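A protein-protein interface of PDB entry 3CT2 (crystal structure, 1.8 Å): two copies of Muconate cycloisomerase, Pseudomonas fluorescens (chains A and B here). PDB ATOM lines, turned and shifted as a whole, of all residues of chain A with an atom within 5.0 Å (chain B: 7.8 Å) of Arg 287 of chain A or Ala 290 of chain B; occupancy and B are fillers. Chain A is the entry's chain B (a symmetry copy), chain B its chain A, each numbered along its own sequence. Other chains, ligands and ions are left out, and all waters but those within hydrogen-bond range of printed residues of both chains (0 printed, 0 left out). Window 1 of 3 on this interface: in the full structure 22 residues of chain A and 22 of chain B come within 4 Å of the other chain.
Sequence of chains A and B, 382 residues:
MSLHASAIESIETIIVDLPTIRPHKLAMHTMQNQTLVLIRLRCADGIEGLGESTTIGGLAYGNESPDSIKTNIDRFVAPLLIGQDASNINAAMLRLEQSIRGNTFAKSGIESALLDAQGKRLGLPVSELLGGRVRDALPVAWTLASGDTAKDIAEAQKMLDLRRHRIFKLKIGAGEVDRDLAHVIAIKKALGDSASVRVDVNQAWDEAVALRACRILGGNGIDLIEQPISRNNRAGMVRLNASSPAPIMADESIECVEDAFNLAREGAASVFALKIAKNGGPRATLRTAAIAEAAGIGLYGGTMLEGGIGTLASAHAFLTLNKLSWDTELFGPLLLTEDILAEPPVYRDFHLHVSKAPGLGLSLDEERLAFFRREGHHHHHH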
ATOM      1  N   VAL A 257      23.789  -2.975 -15.449  1.00  0.00           N
ATOM      2  CA  VAL A 257      23.231  -2.782 -14.118  1.00  0.00           C
ATOM      3  C   VAL A 257      21.699  -2.751 -14.140  1.00  0.00           C
ATOM      4  O   VAL A 257      21.043  -3.310 -13.253  1.00  0.00           O
ATOM      5  CB  VAL A 257      23.758  -1.472 -13.498  1.00  0.00           C
ATOM      6  CG1 VAL A 257      23.075  -1.207 -12.168  1.00  0.00           C
ATOM      7  CG2 VAL A 257      25.273  -1.561 -13.319  1.00  0.00           C
ATOM      8  N   ARG A 283      33.188  -0.882 -10.319  1.00  0.00           N
ATOM      9  CA  ARG A 283      32.211   0.044  -9.751  1.00  0.00           C
ATOM     10  C   ARG A 283      30.774  -0.256 -10.180  1.00  0.00           C
ATOM     11  O   ARG A 283      29.866  -0.285  -9.345  1.00  0.00           O
ATOM     12  CB  ARG A 283      32.603   1.485 -10.097  1.00  0.00           C
ATOM     13  CG  ARG A 283      33.937   1.886  -9.451  1.00  0.00           C
ATOM     14  CD  ARG A 283      34.421   3.270  -9.870  1.00  0.00           C
ATOM     15  NE  ARG A 283      33.475   4.321  -9.528  1.00  0.00           N
ATOM     16  CZ  ARG A 283      32.703   4.942 -10.412  1.00  0.00           C
ATOM     17  NH1 ARG A 283      32.774   4.612 -11.698  1.00  0.00           N
ATOM     18  NH2 ARG A 283      31.865   5.892 -10.015  1.00  0.00           N
ATOM     19  N   ALA A 284      30.566  -0.483 -11.471  1.00  0.00           N
ATOM     20  CA  ALA A 284      29.235  -0.798 -11.978  1.00  0.00           C
ATOM     21  C   ALA A 284      28.770  -2.120 -11.377  1.00  0.00           C
ATOM     22  O   ALA A 284      27.595  -2.298 -11.065  1.00  0.00           O
ATOM     23  CB  ALA A 284      29.261  -0.897 -13.496  1.00  0.00           C
ATOM     24  N   THR A 285      29.703  -3.047 -11.211  1.00  0.00           N
ATOM     25  CA  THR A 285      29.382  -4.346 -10.642  1.00  0.00           C
ATOM     26  C   THR A 285      28.910  -4.206  -9.196  1.00  0.00           C
ATOM     27  O   THR A 285      28.029  -4.943  -8.753  1.00  0.00           O
ATOM     28  CB  THR A 285      30.605  -5.284 -10.719  1.00  0.00           C
ATOM     29  OG1 THR A 285      31.001  -5.416 -12.091  1.00  0.00           O
ATOM     30  CG2 THR A 285      30.266  -6.669 -10.165  1.00  0.00           C
ATOM     31  N   LEU A 286      29.490  -3.262  -8.459  1.00  0.00           N
ATOM     32  CA  LEU A 286      29.077  -3.049  -7.072  1.00  0.00           C
ATOM     33  C   LEU A 286      27.683  -2.412  -7.000  1.00  0.00           C
ATOM     34  O   LEU A 286      26.973  -2.555  -5.996  1.00  0.00           O
ATOM     35  CB  LEU A 286      30.112  -2.200  -6.327  1.00  0.00           C
ATOM     36  CG  LEU A 286      31.420  -2.953  -6.028  1.00  0.00           C
ATOM     37  CD1 LEU A 286      32.408  -2.027  -5.322  1.00  0.00           C
ATOM     38  CD2 LEU A 286      31.120  -4.167  -5.158  1.00  0.00           C
ATOM     39  N   ARG A 287      27.276  -1.713  -8.056  1.00  0.00           N
ATOM     40  CA  ARG A 287      25.937  -1.137  -8.058  1.00  0.00           C
ATOM     41  C   ARG A 287      24.967  -2.295  -8.298  1.00  0.00           C
ATOM     42  O   ARG A 287      23.890  -2.358  -7.705  1.00  0.00           O
ATOM     43  CB  ARG A 287      25.790  -0.068  -9.149  1.00  0.00           C
ATOM     44  CG  ARG A 287      26.585   1.198  -8.851  1.00  0.00           C
ATOM     45  CD  ARG A 287      26.058   2.391  -9.636  1.00  0.00           C
ATOM     46  NE  ARG A 287      26.185   2.218 -11.079  1.00  0.00           N
ATOM     47  CZ  ARG A 287      27.315   2.374 -11.759  1.00  0.00           C
ATOM     48  NH1 ARG A 287      28.436   2.711 -11.128  1.00  0.00           N
ATOM     49  NH2 ARG A 287      27.324   2.193 -13.074  1.00  0.00           N
ATOM     50  N   THR A 288      25.358  -3.224  -9.167  1.00  0.00           N
ATOM     51  CA  THR A 288      24.522  -4.393  -9.429  1.00  0.00           C
ATOM     52  C   THR A 288      24.387  -5.185  -8.122  1.00  0.00           C
ATOM     53  O   THR A 288      23.309  -5.663  -7.780  1.00  0.00           O
ATOM     54  CB  THR A 288      25.136  -5.274 -10.535  1.00  0.00           C
ATOM     55  OG1 THR A 288      24.906  -4.655 -11.811  1.00  0.00           O
ATOM     56  CG2 THR A 288      24.515  -6.674 -10.530  1.00  0.00           C
ATOM     57  N   ALA A 289      25.487  -5.303  -7.383  1.00  0.00           N
ATOM     58  CA  ALA A 289      25.466  -6.013  -6.108  1.00  0.00           C
ATOM     59  C   ALA A 289      24.544  -5.302  -5.114  1.00  0.00           C
ATOM     60  O   ALA A 289      23.820  -5.948  -4.356  1.00  0.00           O
ATOM     61  CB  ALA A 289      26.880  -6.101  -5.534  1.00  0.00           C
ATOM     62  N   ALA A 290      24.573  -3.972  -5.119  1.00  0.00           N
ATOM     63  CA  ALA A 290      23.732  -3.190  -4.214  1.00  0.00           C
ATOM     64  C   ALA A 290      22.256  -3.451  -4.505  1.00  0.00           C
ATOM     65  O   ALA A 290      21.445  -3.573  -3.590  1.00  0.00           O
ATOM     66  CB  ALA A 290      24.044  -1.706  -4.355  1.00  0.00           C
ATOM     67  N   ILE A 291      21.910  -3.538  -5.781  1.00  0.00           N
ATOM     68  CA  ILE A 291      20.530  -3.802  -6.169  1.00  0.00           C
ATOM     69  C   ILE A 291      20.141  -5.202  -5.698  1.00  0.00           C
ATOM     70  O   ILE A 291      19.085  -5.400  -5.094  1.00  0.00           O
ATOM     71  CB  ILE A 291      20.369  -3.700  -7.703  1.00  0.00           C
ATOM     72  CG1 ILE A 291      20.575  -2.243  -8.141  1.00  0.00           C
ATOM     73  CG2 ILE A 291      18.981  -4.215  -8.129  1.00  0.00           C
ATOM     74  CD1 ILE A 291      20.738  -2.063  -9.645  1.00  0.00           C
ATOM     75  N   VAL B 257      17.674   1.683   2.408  1.00  0.00           N
ATOM     76  CA  VAL B 257      17.979   1.383   1.015  1.00  0.00           C
ATOM     77  C   VAL B 257      17.011   0.353   0.432  1.00  0.00           C
ATOM     78  O   VAL B 257      16.581   0.476  -0.713  1.00  0.00           O
ATOM     79  CB  VAL B 257      19.422   0.857   0.872  1.00  0.00           C
ATOM     80  CG1 VAL B 257      19.687   0.439  -0.565  1.00  0.00           C
ATOM     81  CG2 VAL B 257      20.414   1.941   1.306  1.00  0.00           C
ATOM     82  N   ALA B 260      13.861   1.607  -1.022  1.00  0.00           N
ATOM     83  CA  ALA B 260      14.039   2.172  -2.350  1.00  0.00           C
ATOM     84  C   ALA B 260      13.797   1.098  -3.401  1.00  0.00           C
ATOM     85  O   ALA B 260      13.083   1.324  -4.384  1.00  0.00           O
ATOM     86  CB  ALA B 260      15.441   2.748  -2.493  1.00  0.00           C
ATOM     87  N   LEU B 274      16.492  11.922  -1.795  1.00  0.00           N
ATOM     88  CA  LEU B 274      17.668  11.274  -1.224  1.00  0.00           C
ATOM     89  C   LEU B 274      18.080  12.020   0.045  1.00  0.00           C
ATOM     90  O   LEU B 274      18.510  13.178  -0.011  1.00  0.00           O
ATOM     91  CB  LEU B 274      18.829  11.286  -2.229  1.00  0.00           C
ATOM     92  CG  LEU B 274      18.638  10.590  -3.578  1.00  0.00           C
ATOM     93  CD1 LEU B 274      19.861  10.838  -4.462  1.00  0.00           C
ATOM     94  CD2 LEU B 274      18.431   9.099  -3.363  1.00  0.00           C
ATOM     95  N   ARG B 283      27.128   7.117   1.850  1.00  0.00           N
ATOM     96  CA  ARG B 283      27.348   5.886   1.096  1.00  0.00           C
ATOM     97  C   ARG B 283      26.061   5.096   0.864  1.00  0.00           C
ATOM     98  O   ARG B 283      25.789   4.664  -0.257  1.00  0.00           O
ATOM     99  CB  ARG B 283      28.407   5.028   1.795  1.00  0.00           C
ATOM    100  CG  ARG B 283      29.778   5.712   1.799  1.00  0.00           C
ATOM    101  CD  ARG B 283      30.838   4.948   2.592  1.00  0.00           C
ATOM    102  NE  ARG B 283      31.051   3.598   2.083  1.00  0.00           N
ATOM    103  CZ  ARG B 283      30.602   2.496   2.679  1.00  0.00           C
ATOM    104  NH1 ARG B 283      29.914   2.585   3.813  1.00  0.00           N
ATOM    105  NH2 ARG B 283      30.836   1.307   2.139  1.00  0.00           N
ATOM    106  N   ALA B 284      25.264   4.925   1.912  1.00  0.00           N
ATOM    107  CA  ALA B 284      24.002   4.203   1.785  1.00  0.00           C
ATOM    108  C   ALA B 284      23.085   4.968   0.835  1.00  0.00           C
ATOM    109  O   ALA B 284      22.361   4.372   0.041  1.00  0.00           O
ATOM    110  CB  ALA B 284      23.343   4.060   3.154  1.00  0.00           C
ATOM    111  N   THR B 285      23.127   6.294   0.917  1.00  0.00           N
ATOM    112  CA  THR B 285      22.295   7.129   0.059  1.00  0.00           C
ATOM    113  C   THR B 285      22.670   6.945  -1.406  1.00  0.00           C
ATOM    114  O   THR B 285      21.801   6.980  -2.284  1.00  0.00           O
ATOM    115  CB  THR B 285      22.417   8.610   0.468  1.00  0.00           C
ATOM    116  OG1 THR B 285      22.018   8.740   1.839  1.00  0.00           O
ATOM    117  CG2 THR B 285      21.515   9.499  -0.394  1.00  0.00           C
ATOM    118  N   LEU B 286      23.953   6.738  -1.681  1.00  0.00           N
ATOM    119  CA  LEU B 286      24.381   6.528  -3.060  1.00  0.00           C
ATOM    120  C   LEU B 286      23.928   5.161  -3.576  1.00  0.00           C
ATOM    121  O   LEU B 286      23.768   4.973  -4.780  1.00  0.00           O
ATOM    122  CB  LEU B 286      25.896   6.700  -3.192  1.00  0.00           C
ATOM    123  CG  LEU B 286      26.354   8.160  -3.065  1.00  0.00           C
ATOM    124  CD1 LEU B 286      27.869   8.239  -3.148  1.00  0.00           C
ATOM    125  CD2 LEU B 286      25.710   9.008  -4.169  1.00  0.00           C
ATOM    126  N   ARG B 287      23.712   4.203  -2.678  1.00  0.00           N
ATOM    127  CA  ARG B 287      23.218   2.899  -3.120  1.00  0.00           C
ATOM    128  C   ARG B 287      21.742   3.083  -3.481  1.00  0.00           C
ATOM    129  O   ARG B 287      21.251   2.532  -4.471  1.00  0.00           O
ATOM    130  CB  ARG B 287      23.389   1.846  -2.020  1.00  0.00           C
ATOM    131  CG  ARG B 287      24.851   1.477  -1.777  1.00  0.00           C
ATOM    132  CD  ARG B 287      24.992   0.130  -1.075  1.00  0.00           C
ATOM    133  NE  ARG B 287      24.377   0.119   0.248  1.00  0.00           N
ATOM    134  CZ  ARG B 287      24.926   0.644   1.336  1.00  0.00           C
ATOM    135  NH1 ARG B 287      26.120   1.230   1.264  1.00  0.00           N
ATOM    136  NH2 ARG B 287      24.283   0.583   2.496  1.00  0.00           N
ATOM    137  N   THR B 288      21.034   3.874  -2.680  1.00  0.00           N
ATOM    138  CA  THR B 288      19.632   4.148  -2.968  1.00  0.00           C
ATOM    139  C   THR B 288      19.546   4.845  -4.328  1.00  0.00           C
ATOM    140  O   THR B 288      18.675   4.537  -5.140  1.00  0.00           O
ATOM    141  CB  THR B 288      19.008   5.032  -1.869  1.00  0.00           C
ATOM    142  OG1 THR B 288      18.750   4.219  -0.714  1.00  0.00           O
ATOM    143  CG2 THR B 288      17.700   5.662  -2.341  1.00  0.00           C
ATOM    144  N   ALA B 289      20.460   5.776  -4.575  1.00  0.00           N
ATOM    145  CA  ALA B 289      20.493   6.496  -5.845  1.00  0.00           C
ATOM    146  C   ALA B 289      20.770   5.524  -6.993  1.00  0.00           C
ATOM    147  O   ALA B 289      20.192   5.647  -8.070  1.00  0.00           O
ATOM    148  CB  ALA B 289      21.573   7.583  -5.800  1.00  0.00           C
ATOM    149  N   ALA B 290      21.658   4.561  -6.762  1.00  0.00           N
ATOM    150  CA  ALA B 290      21.993   3.580  -7.795  1.00  0.00           C
ATOM    151  C   ALA B 290      20.764   2.755  -8.159  1.00  0.00           C
ATOM    152  O   ALA B 290      20.538   2.442  -9.327  1.00  0.00           O
ATOM    153  CB  ALA B 290      23.111   2.663  -7.311  1.00  0.00           C
ATOM    154  N   ILE B 291      19.966   2.408  -7.155  1.00  0.00           N
ATOM    155  CA  ILE B 291      18.765   1.619  -7.396  1.00  0.00           C
ATOM    156  C   ILE B 291      17.785   2.463  -8.197  1.00  0.00           C
ATOM    157  O   ILE B 291      17.212   2.001  -9.183  1.00  0.00           O
ATOM    158  CB  ILE B 291      18.117   1.184  -6.060  1.00  0.00           C
ATOM    159  CG1 ILE B 291      19.040   0.187  -5.354  1.00  0.00           C
ATOM    160  CG2 ILE B 291      16.737   0.574  -6.309  1.00  0.00           C
ATOM    161  CD1 ILE B 291      18.666  -0.079  -3.905  1.00  0.00           C
ATOM    162  N   ALA B 292      17.603   3.713  -7.782  1.00  0.00           N
ATOM    163  CA  ALA B 292      16.682   4.599  -8.487  1.00  0.00           C
ATOM    164  C   ALA B 292      17.096   4.774  -9.948  1.00  0.00           C
ATOM    165  O   ALA B 292      16.269   4.652 -10.854  1.00  0.00           O
ATOM    166  CB  ALA B 292      16.619   5.946  -7.784  1.00  0.00           C
ATOM    167  N   GLU B 293      18.378   5.050 -10.180  1.00  0.00           N
ATOM    168  CA  GLU B 293      18.883   5.236 -11.541  1.00  0.00           C
ATOM    169  C   GLU B 293      18.661   3.991 -12.401  1.00  0.00           C
ATOM    170  O   GLU B 293      18.254   4.088 -13.556  1.00  0.00           O
ATOM    171  CB  GLU B 293      20.376   5.556 -11.518  1.00  0.00           C
ATOM    172  CG  GLU B 293      20.746   6.775 -10.717  1.00  0.00           C
ATOM    173  CD  GLU B 293      22.245   6.926 -10.586  1.00  0.00           C
ATOM    174  OE1 GLU B 293      22.936   5.885 -10.483  1.00  0.00           O
ATOM    175  OE2 GLU B 293      22.734   8.073 -10.579  1.00  0.00           O
ATOM    176  N   ALA B 294      18.929   2.821 -11.832  1.00  0.00           N
ATOM    177  CA  ALA B 294      18.755   1.569 -12.569  1.00  0.00           C
ATOM    178  C   ALA B 294      17.294   1.336 -12.924  1.00  0.00           C
ATOM    179  O   ALA B 294      16.992   0.613 -13.872  1.00  0.00           O
ATOM    180  CB  ALA B 294      19.284   0.398 -11.752  1.00  0.00           C
ATOM    181  N   ALA B 295      16.390   1.943 -12.159  1.00  0.00           N
ATOM    182  CA  ALA B 295      14.958   1.790 -12.393  1.00  0.00           C
ATOM    183  C   ALA B 295      14.371   2.922 -13.237  1.00  0.00           C
ATOM    184  O   ALA B 295      13.170   2.916 -13.539  1.00  0.00           O
ATOM    185  CB  ALA B 295      14.218   1.711 -11.055  1.00  0.00           C
ATOM    186  N   GLY B 296      15.206   3.891 -13.603  1.00  0.00           N
ATOM    187  CA  GLY B 296      14.734   5.016 -14.398  1.00  0.00           C
ATOM    188  C   GLY B 296      13.984   6.047 -13.568  1.00  0.00           C
ATOM    189  O   GLY B 296      13.207   6.849 -14.096  1.00  0.00           O
ATOM    190  N   ILE B 297      14.220   6.030 -12.261  1.00  0.00           N
ATOM    191  CA  ILE B 297      13.568   6.951 -11.337  1.00  0.00           C
ATOM    192  C   ILE B 297      14.419   8.206 -11.116  1.00  0.00           C
ATOM    193  O   ILE B 297      15.634   8.115 -10.929  1.00  0.00           O
ATOM    194  CB  ILE B 297      13.294   6.235  -9.989  1.00  0.00           C
ATOM    195  CG1 ILE B 297      12.259   5.119 -10.218  1.00  0.00           C
ATOM    196  CG2 ILE B 297      12.789   7.231  -8.946  1.00  0.00           C
ATOM    197  CD1 ILE B 297      12.000   4.233  -9.000  1.00  0.00           C
ATOM    198  N   LEU B 299      16.018  11.714  -9.441  1.00  0.00           N
ATOM    199  CA  LEU B 299      16.613  11.983  -8.139  1.00  0.00           C
ATOM    200  C   LEU B 299      16.448  13.423  -7.661  1.00  0.00           C
ATOM    201  O   LEU B 299      16.419  14.363  -8.458  1.00  0.00           O
ATOM    202  CB  LEU B 299      18.102  11.628  -8.158  1.00  0.00           C
ATOM    203  CG  LEU B 299      18.450  10.204  -8.599  1.00  0.00           C
ATOM    204  CD1 LEU B 299      19.959  10.024  -8.595  1.00  0.00           C
ATOM    205  CD2 LEU B 299      17.794   9.202  -7.657  1.00  0.00           C
ATOM    206  N   LEU B 321      26.613  12.257  -8.468  1.00  0.00           N
ATOM    207  CA  LEU B 321      25.509  11.713  -9.256  1.00  0.00           C
ATOM    208  C   LEU B 321      25.510  12.207 -10.695  1.00  0.00           C
ATOM    209  O   LEU B 321      25.642  13.404 -10.944  1.00  0.00           O
ATOM    210  CB  LEU B 321      24.173  12.068  -8.597  1.00  0.00           C
ATOM    211  CG  LEU B 321      23.979  11.474  -7.199  1.00  0.00           C
ATOM    212  CD1 LEU B 321      22.695  12.016  -6.580  1.00  0.00           C
ATOM    213  CD2 LEU B 321      23.946   9.954  -7.300  1.00  0.00           C
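Arg 287 of chain A touches just one residue of chain B: Ala 290 (3.8 Å). Of chain A, only Arg 287 comes within 4 Å of Ala 290 of chain B. Of the printed residues of chain A, Ala 294 of chain B touches Ile 291 (3.6 Å). Printed residues of chain B within 4 Å of Ile 291 of chain A: Ala 294. Printed residues of chain A within 4 Å of Arg 287 of chain B: Ala 290. Printed residues of chain B within 4 Å of Ala 290 of chain A: Arg 287. Leu 321 of chain B touches none of the printed residues of chain A. The nearest residue of chain B that does not touch Arg 287 of chain A is Glu 293 of chain B (4.8 Å). The nearest residue of chain A that does not touch Ala 290 of chain B is Ile 291 of chain A (4.5 Å).
Of the 10 printed residues of chain A, 3 touch a printed residue of chain B. Printed residues of chain A that touch a printed residue of chain B: Arg 287, Ala 290 and Ile 291. Hydrophobic or aromatic side chains of chain A within 4 Å of the printed part of chain B: Ala 290 and Ile 291. Along chain A the printed residues that touch a printed residue of chain B span positions 287 to 291. Of the 20 printed residues of chain B, 3 touch a printed residue of chain A. Printed residues of chain B that touch a printed residue of chain A: Arg 287, Ala 290 and Ala 294. Hydrophobic or aromatic side chains of chain B that line the printed part of chain A: Ala 290 and Ala 294. Among the printed residues, 3 pairs touch across the chains.
CD of Arg 287 of chain A touches CB of Ala 290 of chain B, 3.8 Å away. Arg 287 of chain B touches Ala 290 of chain A. Ala 294 of chain B touches Ile 291 of chain A.
Arg 287 of chain A touches Ala 290 of chain B, and with the chains exchanged Ala 290 of chain A touches Arg 287 of chain B. Positions printed for both chains: 257, 283, 284, 285, 286, 287, 288, 289, 290 and 291.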
